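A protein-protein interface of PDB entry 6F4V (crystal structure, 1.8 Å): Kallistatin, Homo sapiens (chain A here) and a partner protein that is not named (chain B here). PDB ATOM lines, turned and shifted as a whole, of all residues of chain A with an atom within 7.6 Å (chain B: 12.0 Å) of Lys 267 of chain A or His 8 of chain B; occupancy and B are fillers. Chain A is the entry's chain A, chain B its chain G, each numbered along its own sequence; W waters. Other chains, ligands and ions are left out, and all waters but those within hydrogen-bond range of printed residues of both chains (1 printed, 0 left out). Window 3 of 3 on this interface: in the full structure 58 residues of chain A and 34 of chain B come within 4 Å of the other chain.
OH of Tyr 209 of chain A lies within hydrogen-bond range of ND1 of His 8 of chain B (2.9 Å).
The backbone carbonyl oxygen (O) of Arg 7 of chain B lies within hydrogen-bond range of a ring nitrogen (NE2) of His 211 of chain A (2.8 Å).
The backbone NH (N) of Glu 269 of chain A sits at hydrogen-bond distance from the backbone carbonyl oxygen (O) of His 8 of chain B, at 2.9 Å.
The backbone NH of Leu 10 of chain B sits at hydrogen-bond distance from the backbone carbonyl oxygen of Glu 269 of chain A, at 2.9 Å.
NH2 of Arg 11 of chain B is in salt-bridge range of OE2 of Glu 269 of chain A.
The backbone NH of Leu 270 of chain A sits at hydrogen-bond distance from the backbone carbonyl oxygen of Gln 202 of chain A, 2.9 Å away.
The backbone NH of Leu 268 of chain A is in hydrogen-bond range of the backbone carbonyl oxygen of Glu 205 of chain A, 3.3 Å away.
The backbone carbonyl oxygen of Phe 264 of chain A sits at hydrogen-bond distance from the backbone NH of Tyr 209 of chain A.
OH of Tyr 209 of chain A lies within hydrogen-bond range of O of Lys 267 of chain A, 2.8 Å away.
CE2 of Tyr 209 of chain A touches O of Arg 7 of chain B, 3.6 Å away.
CD2 of Leu 10 of chain B touches CE1 of His 211 of chain A (3.8 Å).
CB of His 8 of chain B touches O of Lys 267 of chain A, 3.6 Å away.
His 8 of chain B touches Leu 268 of chain A.
Ile 9 of chain B touches Leu 268 of chain A (C to CD1, 3.9 Å).
Leu 10 of chain B touches Leu 268 of chain A (N to CD1, 3.7 Å).
OE2 of Glu 269 of chain A touches CD1 of Ile 9 of chain B (3.1 Å).
O of Leu 10 of chain B touches CA of Leu 270 of chain A, at 3.6 Å.
Phe 12 of chain B touches Leu 270 of chain A.
Of chain A, only Tyr 209 (2.9 Å), Lys 267 (3.6 Å), Leu 268 (3.6 Å) and Glu 269 (2.9 Å) come within 4 Å of His 8 of chain B.
No residue of chain B comes within 4 Å of Gln 204 of chain A.
No residue of chain B comes within 4 Å of His 206 of chain A.
No residue of chain B comes within 4 Å of Lys 266 of chain A.
Leu 268 of chain A touches just these residues of chain B: His 8 (3.6 Å), Ile 9 (3.9 Å) and Leu 10 (3.7 Å).
Printed residues of chain A within 4 Å of Ile 9 of chain B: Leu 268 and Glu 269.
Printed residues of chain B within 4 Å of His 211 of chain A: Arg 7 (2.8 Å) and Leu 10 (3.8 Å).
Trp 208 of chain A touches none of the printed residues of chain B.
Asp 203 of chain A touches none of the printed residues of chain B.
The nearest residue of chain A that does not touch His 8 of chain B is Lys 266 of chain A (4.4 Å).
The nearest printed residue of chain A that does not touch Phe 12 of chain B is Leu 268 of chain A (6.4 Å).
Of the 8 printed residues of chain B, 6 touch a printed residue of chain A.
Of the 17 printed residues of chain A, 6 touch a printed residue of chain B.
Hydrophobic or aromatic side chains of chain A within 4 Å of the printed part of chain B: Tyr 209, His 211, Leu 268 and Leu 270.
Along chain A the printed residues that touch a printed residue of chain B span positions 209 to 270.
Among the printed residues, 14 pairs touch across the chains.
Water W1 lies within hydrogen-bond range of the backbone carbonyl oxygen of His 8 of chain B and the backbone NH of Glu 269 of chain A.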
ATOM      1  N   GLN A 202     -20.034  -0.621  33.764  1.00  0.00           N
ATOM      2  CA  GLN A 202     -19.189  -1.775  33.996  1.00  0.00           C
ATOM      3  C   GLN A 202     -19.276  -2.660  32.774  1.00  0.00           C
ATOM      4  O   GLN A 202     -20.320  -2.760  32.171  1.00  0.00           O
ATOM      5  CB  GLN A 202     -19.524  -2.557  35.289  1.00  0.00           C
ATOM      6  CG  GLN A 202     -20.910  -3.124  35.415  1.00  0.00           C
ATOM      7  CD  GLN A 202     -21.084  -3.919  36.682  1.00  0.00           C
ATOM      8  OE1 GLN A 202     -20.618  -5.054  36.774  1.00  0.00           O
ATOM      9  NE2 GLN A 202     -21.767  -3.340  37.667  1.00  0.00           N
ATOM     10  N   ASP A 203     -18.146  -3.267  32.399  1.00  0.00           N
ATOM     11  CA  ASP A 203     -18.086  -4.134  31.219  1.00  0.00           C
ATOM     12  C   ASP A 203     -17.210  -5.394  31.346  1.00  0.00           C
ATOM     13  O   ASP A 203     -17.019  -6.102  30.352  1.00  0.00           O
ATOM     14  CB  ASP A 203     -17.683  -3.317  30.007  1.00  0.00           C
ATOM     15  CG  ASP A 203     -16.319  -2.639  30.172  1.00  0.00           C
ATOM     16  OD1 ASP A 203     -15.576  -2.943  31.125  1.00  0.00           O
ATOM     17  OD2 ASP A 203     -16.003  -1.766  29.356  1.00  0.00           O
ATOM     18  N   GLN A 204     -16.729  -5.708  32.542  1.00  0.00           N
ATOM     19  CA  GLN A 204     -15.878  -6.893  32.722  1.00  0.00           C
ATOM     20  C   GLN A 204     -16.605  -8.064  33.355  1.00  0.00           C
ATOM     21  O   GLN A 204     -16.085  -9.185  33.344  1.00  0.00           O
ATOM     22  CB  GLN A 204     -14.610  -6.546  33.530  1.00  0.00           C
ATOM     23  CG  GLN A 204     -13.861  -5.277  33.098  1.00  0.00           C
ATOM     24  CD  GLN A 204     -13.241  -5.329  31.708  1.00  0.00           C
ATOM     25  OE1 GLN A 204     -12.048  -5.101  31.561  1.00  0.00           O
ATOM     26  NE2 GLN A 204     -14.043  -5.594  30.687  1.00  0.00           N
ATOM     27  N   GLU A 205     -17.812  -7.832  33.882  1.00  0.00           N
ATOM     28  CA  GLU A 205     -18.498  -8.846  34.667  1.00  0.00           C
ATOM     29  C   GLU A 205     -19.525  -9.601  33.838  1.00  0.00           C
ATOM     30  O   GLU A 205     -20.033  -9.079  32.857  1.00  0.00           O
ATOM     31  CB  GLU A 205     -19.220  -8.198  35.833  1.00  0.00           C
ATOM     32  CG  GLU A 205     -18.321  -7.429  36.774  1.00  0.00           C
ATOM     33  CD  GLU A 205     -17.335  -8.334  37.471  1.00  0.00           C
ATOM     34  OE1 GLU A 205     -17.783  -9.295  38.137  1.00  0.00           O
ATOM     35  OE2 GLU A 205     -16.121  -8.089  37.333  1.00  0.00           O
ATOM     36  N   HIS A 206     -19.804 -10.837  34.245  1.00  0.00           N
ATOM     37  CA  HIS A 206     -20.983 -11.560  33.758  1.00  0.00           C
ATOM     38  C   HIS A 206     -22.180 -11.065  34.548  1.00  0.00           C
ATOM     39  O   HIS A 206     -22.053 -10.774  35.726  1.00  0.00           O
ATOM     40  CB  HIS A 206     -20.843 -13.062  33.939  1.00  0.00           C
ATOM     41  CG  HIS A 206     -20.013 -13.727  32.880  1.00  0.00           C
ATOM     42  ND1 HIS A 206     -18.788 -13.242  32.480  1.00  0.00           N
ATOM     43  CD2 HIS A 206     -20.239 -14.840  32.136  1.00  0.00           C
ATOM     44  CE1 HIS A 206     -18.300 -14.016  31.522  1.00  0.00           C
ATOM     45  NE2 HIS A 206     -19.159 -14.996  31.300  1.00  0.00           N
ATOM     46  N   HIS A 207     -23.329 -10.987  33.886  1.00  0.00           N
ATOM     47  CA  HIS A 207     -24.591 -10.619  34.520  1.00  0.00           C
ATOM     48  C   HIS A 207     -25.710 -11.542  34.071  1.00  0.00           C
ATOM     49  O   HIS A 207     -25.597 -12.184  33.020  1.00  0.00           O
ATOM     50  CB  HIS A 207     -24.926  -9.180  34.122  1.00  0.00           C
ATOM     51  CG  HIS A 207     -24.187  -8.163  34.916  1.00  0.00           C
ATOM     52  ND1 HIS A 207     -24.600  -7.762  36.168  1.00  0.00           N
ATOM     53  CD2 HIS A 207     -23.035  -7.499  34.658  1.00  0.00           C
ATOM     54  CE1 HIS A 207     -23.745  -6.874  36.637  1.00  0.00           C
ATOM     55  NE2 HIS A 207     -22.792  -6.692  35.739  1.00  0.00           N
ATOM     56  N   TRP A 208     -26.793 -11.583  34.864  1.00  0.00           N
ATOM     57  CA  TRP A 208     -27.979 -12.363  34.560  1.00  0.00           C
ATOM     58  C   TRP A 208     -28.905 -11.444  33.802  1.00  0.00           C
ATOM     59  O   TRP A 208     -29.434 -10.480  34.393  1.00  0.00           O
ATOM     60  CB  TRP A 208     -28.647 -12.839  35.848  1.00  0.00           C
ATOM     61  CG  TRP A 208     -27.860 -13.824  36.582  1.00  0.00           C
ATOM     62  CD1 TRP A 208     -27.001 -13.600  37.624  1.00  0.00           C
ATOM     63  CD2 TRP A 208     -27.860 -15.223  36.352  1.00  0.00           C
ATOM     64  NE1 TRP A 208     -26.468 -14.794  38.060  1.00  0.00           N
ATOM     65  CE2 TRP A 208     -26.983 -15.806  37.294  1.00  0.00           C
ATOM     66  CE3 TRP A 208     -28.524 -16.048  35.443  1.00  0.00           C
ATOM     67  CZ2 TRP A 208     -26.737 -17.193  37.336  1.00  0.00           C
ATOM     68  CZ3 TRP A 208     -28.287 -17.430  35.499  1.00  0.00           C
ATOM     69  CH2 TRP A 208     -27.423 -17.978  36.442  1.00  0.00           C
ATOM     70  N   TYR A 209     -29.056 -11.672  32.496  1.00  0.00           N
ATOM     71  CA  TYR A 209     -29.962 -10.854  31.684  1.00  0.00           C
ATOM     72  C   TYR A 209     -30.508 -11.611  30.484  1.00  0.00           C
ATOM     73  O   TYR A 209     -29.945 -12.615  30.057  1.00  0.00           O
ATOM     74  CB  TYR A 209     -29.297  -9.535  31.225  1.00  0.00           C
ATOM     75  CG  TYR A 209     -28.148  -9.731  30.240  1.00  0.00           C
ATOM     76  CD1 TYR A 209     -26.904 -10.181  30.677  1.00  0.00           C
ATOM     77  CD2 TYR A 209     -28.318  -9.471  28.876  1.00  0.00           C
ATOM     78  CE1 TYR A 209     -25.858 -10.367  29.785  1.00  0.00           C
ATOM     79  CE2 TYR A 209     -27.283  -9.661  27.971  1.00  0.00           C
ATOM     80  CZ  TYR A 209     -26.051 -10.113  28.441  1.00  0.00           C
ATOM     81  OH  TYR A 209     -25.013 -10.280  27.568  1.00  0.00           O
ATOM     82  N   HIS A 211     -32.976 -10.889  26.664  1.00  0.00           N
ATOM     83  CA  HIS A 211     -33.792 -10.104  25.738  1.00  0.00           C
ATOM     84  C   HIS A 211     -35.025 -10.947  25.481  1.00  0.00           C
ATOM     85  O   HIS A 211     -34.934 -12.059  24.925  1.00  0.00           O
ATOM     86  CB  HIS A 211     -33.009  -9.810  24.452  1.00  0.00           C
ATOM     87  CG  HIS A 211     -31.661  -9.199  24.688  1.00  0.00           C
ATOM     88  ND1 HIS A 211     -31.492  -7.945  25.242  1.00  0.00           N
ATOM     89  CD2 HIS A 211     -30.408  -9.667  24.435  1.00  0.00           C
ATOM     90  CE1 HIS A 211     -30.198  -7.664  25.312  1.00  0.00           C
ATOM     91  NE2 HIS A 211     -29.520  -8.694  24.831  1.00  0.00           N
ATOM     92  N   ASN A 263     -27.273 -20.276  30.711  1.00  0.00           N
ATOM     93  CA  ASN A 263     -27.198 -19.629  29.396  1.00  0.00           C
ATOM     94  C   ASN A 263     -27.635 -18.158  29.375  1.00  0.00           C
ATOM     95  O   ASN A 263     -27.353 -17.461  28.405  1.00  0.00           O
ATOM     96  CB  ASN A 263     -27.924 -20.418  28.315  1.00  0.00           C
ATOM     97  CG  ASN A 263     -29.386 -20.184  28.311  1.00  0.00           C
ATOM     98  OD1 ASN A 263     -29.900 -19.434  27.464  1.00  0.00           O
ATOM     99  ND2 ASN A 263     -30.091 -20.803  29.261  1.00  0.00           N
ATOM    100  N   PHE A 264     -28.284 -17.677  30.445  1.00  0.00           N
ATOM    101  CA  PHE A 264     -28.575 -16.247  30.574  1.00  0.00           C
ATOM    102  C   PHE A 264     -27.585 -15.507  31.476  1.00  0.00           C
ATOM    103  O   PHE A 264     -27.814 -14.363  31.843  1.00  0.00           O
ATOM    104  CB  PHE A 264     -30.041 -16.062  30.999  1.00  0.00           C
ATOM    105  CG  PHE A 264     -31.020 -16.495  29.940  1.00  0.00           C
ATOM    106  CD1 PHE A 264     -31.173 -15.749  28.780  1.00  0.00           C
ATOM    107  CD2 PHE A 264     -31.776 -17.640  30.089  1.00  0.00           C
ATOM    108  CE1 PHE A 264     -32.064 -16.152  27.784  1.00  0.00           C
ATOM    109  CE2 PHE A 264     -32.667 -18.053  29.101  1.00  0.00           C
ATOM    110  CZ  PHE A 264     -32.820 -17.300  27.949  1.00  0.00           C
ATOM    111  N   TYR A 265     -26.448 -16.137  31.786  1.00  0.00           N
ATOM    112  CA  TYR A 265     -25.376 -15.509  32.545  1.00  0.00           C
ATOM    113  C   TYR A 265     -24.229 -15.301  31.583  1.00  0.00           C
ATOM    114  O   TYR A 265     -23.526 -16.246  31.241  1.00  0.00           O
ATOM    115  CB  TYR A 265     -24.991 -16.388  33.718  1.00  0.00           C
ATOM    116  CG  TYR A 265     -23.981 -15.814  34.673  1.00  0.00           C
ATOM    117  CD1 TYR A 265     -24.327 -14.772  35.536  1.00  0.00           C
ATOM    118  CD2 TYR A 265     -22.681 -16.351  34.766  1.00  0.00           C
ATOM    119  CE1 TYR A 265     -23.413 -14.254  36.441  1.00  0.00           C
ATOM    120  CE2 TYR A 265     -21.755 -15.841  35.672  1.00  0.00           C
ATOM    121  CZ  TYR A 265     -22.133 -14.789  36.510  1.00  0.00           C
ATOM    122  OH  TYR A 265     -21.244 -14.273  37.404  1.00  0.00           O
ATOM    123  N   LYS A 266     -24.082 -14.069  31.115  1.00  0.00           N
ATOM    124  CA  LYS A 266     -23.149 -13.733  30.040  1.00  0.00           C
ATOM    125  C   LYS A 266     -22.421 -12.448  30.372  1.00  0.00           C
ATOM    126  O   LYS A 266     -22.900 -11.640  31.191  1.00  0.00           O
ATOM    127  CB  LYS A 266     -23.895 -13.537  28.719  1.00  0.00           C
ATOM    128  CG  LYS A 266     -24.631 -14.766  28.186  1.00  0.00           C
ATOM    129  CD  LYS A 266     -23.643 -15.815  27.674  1.00  0.00           C
ATOM    130  CE  LYS A 266     -24.339 -17.104  27.247  1.00  0.00           C
ATOM    131  NZ  LYS A 266     -25.393 -16.821  26.236  1.00  0.00           N
ATOM    132  N   LYS A 267     -21.283 -12.227  29.703  1.00  0.00           N
ATOM    133  CA  LYS A 267     -20.600 -10.935  29.794  1.00  0.00           C
ATOM    134  C   LYS A 267     -21.565  -9.852  29.303  1.00  0.00           C
ATOM    135  O   LYS A 267     -22.393 -10.066  28.406  1.00  0.00           O
ATOM    136  CB  LYS A 267     -19.247 -10.886  29.041  1.00  0.00           C
ATOM    137  CG  LYS A 267     -18.413  -9.654  29.424  1.00  0.00           C
ATOM    138  CD  LYS A 267     -16.957  -9.669  28.924  1.00  0.00           C
ATOM    139  CE  LYS A 267     -15.964 -10.109  30.006  1.00  0.00           C
ATOM    140  NZ  LYS A 267     -14.540  -9.770  29.683  1.00  0.00           N
ATOM    141  N   LEU A 268     -21.519  -8.720  29.986  1.00  0.00           N
ATOM    142  CA  LEU A 268     -22.393  -7.619  29.676  1.00  0.00           C
ATOM    143  C   LEU A 268     -21.663  -6.298  29.774  1.00  0.00           C
ATOM    144  O   LEU A 268     -20.982  -6.031  30.760  1.00  0.00           O
ATOM    145  CB  LEU A 268     -23.550  -7.600  30.656  1.00  0.00           C
ATOM    146  CG  LEU A 268     -24.565  -6.478  30.524  1.00  0.00           C
ATOM    147  CD1 LEU A 268     -25.326  -6.640  29.239  1.00  0.00           C
ATOM    148  CD2 LEU A 268     -25.546  -6.491  31.695  1.00  0.00           C
ATOM    149  N   GLU A 269     -21.883  -5.456  28.783  1.00  0.00           N
ATOM    150  CA  GLU A 269     -21.547  -4.053  28.887  1.00  0.00           C
ATOM    151  C   GLU A 269     -22.802  -3.342  29.390  1.00  0.00           C
ATOM    152  O   GLU A 269     -23.788  -3.289  28.674  1.00  0.00           O
ATOM    153  CB  GLU A 269     -21.125  -3.514  27.526  1.00  0.00           C
ATOM    154  CG  GLU A 269     -20.679  -2.065  27.527  1.00  0.00           C
ATOM    155  CD  GLU A 269     -20.599  -1.515  26.102  1.00  0.00           C
ATOM    156  OE1 GLU A 269     -20.153  -2.275  25.219  1.00  0.00           O
ATOM    157  OE2 GLU A 269     -21.015  -0.365  25.842  1.00  0.00           O
ATOM    158  N   LEU A 270     -22.741  -2.819  30.613  1.00  0.00           N
ATOM    159  CA  LEU A 270     -23.918  -2.304  31.328  1.00  0.00           C
ATOM    160  C   LEU A 270     -23.747  -0.827  31.608  1.00  0.00           C
ATOM    161  O   LEU A 270     -22.792  -0.430  32.265  1.00  0.00           O
ATOM    162  CB  LEU A 270     -24.090  -3.058  32.657  1.00  0.00           C
ATOM    163  CG  LEU A 270     -25.173  -2.559  33.608  1.00  0.00           C
ATOM    164  CD1 LEU A 270     -26.532  -2.558  32.928  1.00  0.00           C
ATOM    165  CD2 LEU A 270     -25.203  -3.437  34.836  1.00  0.00           C
ATOM    166  N   ASN B   6     -25.369  -6.357  18.557  1.00  0.00           N
ATOM    167  CA  ASN B   6     -24.902  -5.885  19.905  1.00  0.00           C
ATOM    168  C   ASN B   6     -25.729  -6.533  21.043  1.00  0.00           C
ATOM    169  O   ASN B   6     -26.348  -5.837  21.843  1.00  0.00           O
ATOM    170  CB  ASN B   6     -24.993  -4.343  19.996  1.00  0.00           C
ATOM    171  CG  ASN B   6     -24.161  -3.622  18.938  1.00  0.00           C
ATOM    172  OD1 ASN B   6     -22.939  -3.813  18.843  1.00  0.00           O
ATOM    173  ND2 ASN B   6     -24.816  -2.757  18.157  1.00  0.00           N
ATOM    174  N   ARG B   7     -25.734  -7.864  21.125  1.00  0.00           N
ATOM    175  CA  ARG B   7     -26.614  -8.567  22.078  1.00  0.00           C
ATOM    176  C   ARG B   7     -26.079  -8.613  23.523  1.00  0.00           C
ATOM    177  O   ARG B   7     -26.815  -9.005  24.434  1.00  0.00           O
ATOM    178  CB  ARG B   7     -26.943  -9.982  21.574  1.00  0.00           C
ATOM    179  CG  ARG B   7     -28.010  -9.993  20.481  1.00  0.00           C
ATOM    180  CD  ARG B   7     -28.364 -11.409  20.032  1.00  0.00           C
ATOM    181  NE  ARG B   7     -29.034 -12.203  21.073  1.00  0.00           N
ATOM    182  CZ  ARG B   7     -30.318 -12.088  21.445  1.00  0.00           C
ATOM    183  NH1 ARG B   7     -30.798 -12.885  22.405  1.00  0.00           N
ATOM    184  NH2 ARG B   7     -31.134 -11.185  20.882  1.00  0.00           N
ATOM    185  N   HIS B   8     -24.816  -8.220  23.727  1.00  0.00           N
ATOM    186  CA  HIS B   8     -24.173  -8.220  25.049  1.00  0.00           C
ATOM    187  C   HIS B   8     -24.000  -6.823  25.632  1.00  0.00           C
ATOM    188  O   HIS B   8     -23.039  -6.549  26.346  1.00  0.00           O
ATOM    189  CB  HIS B   8     -22.826  -8.959  24.979  1.00  0.00           C
ATOM    190  CG  HIS B   8     -22.962 -10.395  24.599  1.00  0.00           C
ATOM    191  ND1 HIS B   8     -24.034 -11.165  24.996  1.00  0.00           N
ATOM    192  CD2 HIS B   8     -22.179 -11.201  23.848  1.00  0.00           C
ATOM    193  CE1 HIS B   8     -23.895 -12.389  24.521  1.00  0.00           C
ATOM    194  NE2 HIS B   8     -22.775 -12.438  23.824  1.00  0.00           N
ATOM    195  N   ILE B   9     -24.961  -5.951  25.349  1.00  0.00           N
ATOM    196  CA  ILE B   9     -24.966  -4.592  25.868  1.00  0.00           C
ATOM    197  C   ILE B   9     -26.375  -4.209  26.351  1.00  0.00           C
ATOM    198  O   ILE B   9     -27.374  -4.535  25.714  1.00  0.00           O
ATOM    199  CB  ILE B   9     -24.454  -3.582  24.822  1.00  0.00           C
ATOM    200  CG1 ILE B   9     -24.480  -2.161  25.376  1.00  0.00           C
ATOM    201  CG2 ILE B   9     -25.304  -3.629  23.575  1.00  0.00           C
ATOM    202  CD1 ILE B   9     -23.681  -1.184  24.565  1.00  0.00           C
ATOM    203  N   LEU B  10     -26.435  -3.520  27.485  1.00  0.00           N
ATOM    204  CA  LEU B  10     -27.655  -2.904  27.937  1.00  0.00           C
ATOM    205  C   LEU B  10     -27.367  -1.469  28.321  1.00  0.00           C
ATOM    206  O   LEU B  10     -26.496  -1.209  29.143  1.00  0.00           O
ATOM    207  CB  LEU B  10     -28.248  -3.671  29.127  1.00  0.00           C
ATOM    208  CG  LEU B  10     -28.944  -4.989  28.777  1.00  0.00           C
ATOM    209  CD1 LEU B  10     -29.385  -5.702  30.034  1.00  0.00           C
ATOM    210  CD2 LEU B  10     -30.132  -4.815  27.855  1.00  0.00           C
ATOM    211  N   ARG B  11     -28.131  -0.547  27.751  1.00  0.00           N
ATOM    212  CA  ARG B  11     -28.062   0.861  28.098  1.00  0.00           C
ATOM    213  C   ARG B  11     -29.361   1.314  28.693  1.00  0.00           C
ATOM    214  O   ARG B  11     -30.353   1.419  27.994  1.00  0.00           O
ATOM    215  CB  ARG B  11     -27.810   1.728  26.848  1.00  0.00           C
ATOM    216  CG  ARG B  11     -26.519   1.466  26.159  1.00  0.00           C
ATOM    217  CD  ARG B  11     -26.459   2.328  24.894  1.00  0.00           C
ATOM    218  NE  ARG B  11     -25.238   2.056  24.132  1.00  0.00           N
ATOM    219  CZ  ARG B  11     -24.049   2.584  24.407  1.00  0.00           C
ATOM    220  NH1 ARG B  11     -23.884   3.418  25.442  1.00  0.00           N
ATOM    221  NH2 ARG B  11     -23.005   2.268  23.642  1.00  0.00           N
ATOM    222  N   PHE B  12     -29.356   1.597  29.996  1.00  0.00           N
ATOM    223  CA  PHE B  12     -30.535   2.107  30.656  1.00  0.00           C
ATOM    224  C   PHE B  12     -30.609   3.633  30.483  1.00  0.00           C
ATOM    225  O   PHE B  12     -30.422   4.398  31.417  1.00  0.00           O
ATOM    226  CB  PHE B  12     -30.577   1.638  32.110  1.00  0.00           C
ATOM    227  CG  PHE B  12     -30.892   0.182  32.252  1.00  0.00           C
ATOM    228  CD1 PHE B  12     -29.900  -0.781  32.085  1.00  0.00           C
ATOM    229  CD2 PHE B  12     -32.193  -0.242  32.577  1.00  0.00           C
ATOM    230  CE1 PHE B  12     -30.194  -2.126  32.232  1.00  0.00           C
ATOM    231  CE2 PHE B  12     -32.495  -1.594  32.692  1.00  0.00           C
ATOM    232  CZ  PHE B  12     -31.503  -2.544  32.513  1.00  0.00           C
ATOM    233  N   ARG B  14     -33.292   5.119  28.800  1.00  0.00           N
ATOM    234  CA  ARG B  14     -34.688   5.412  28.504  1.00  0.00           C
ATOM    235  C   ARG B  14     -35.494   4.821  29.667  1.00  0.00           C
ATOM    236  O   ARG B  14     -34.926   4.063  30.445  1.00  0.00           O
ATOM    237  CB  ARG B  14     -35.107   4.815  27.147  1.00  0.00           C
ATOM    238  CG  ARG B  14     -34.901   3.320  27.013  1.00  0.00           C
ATOM    239  CD  ARG B  14     -35.515   2.807  25.714  1.00  0.00           C
ATOM    240  NE  ARG B  14     -35.225   1.389  25.481  1.00  0.00           N
ATOM    241  CZ  ARG B  14     -34.045   0.920  25.113  1.00  0.00           C
ATOM    242  NH1 ARG B  14     -33.010   1.738  24.931  1.00  0.00           N
ATOM    243  NH2 ARG B  14     -33.883  -0.380  24.918  1.00  0.00           N
HETATM  244  O   HOH W   1     -20.206  -7.377  26.489  1.00  0.00           O
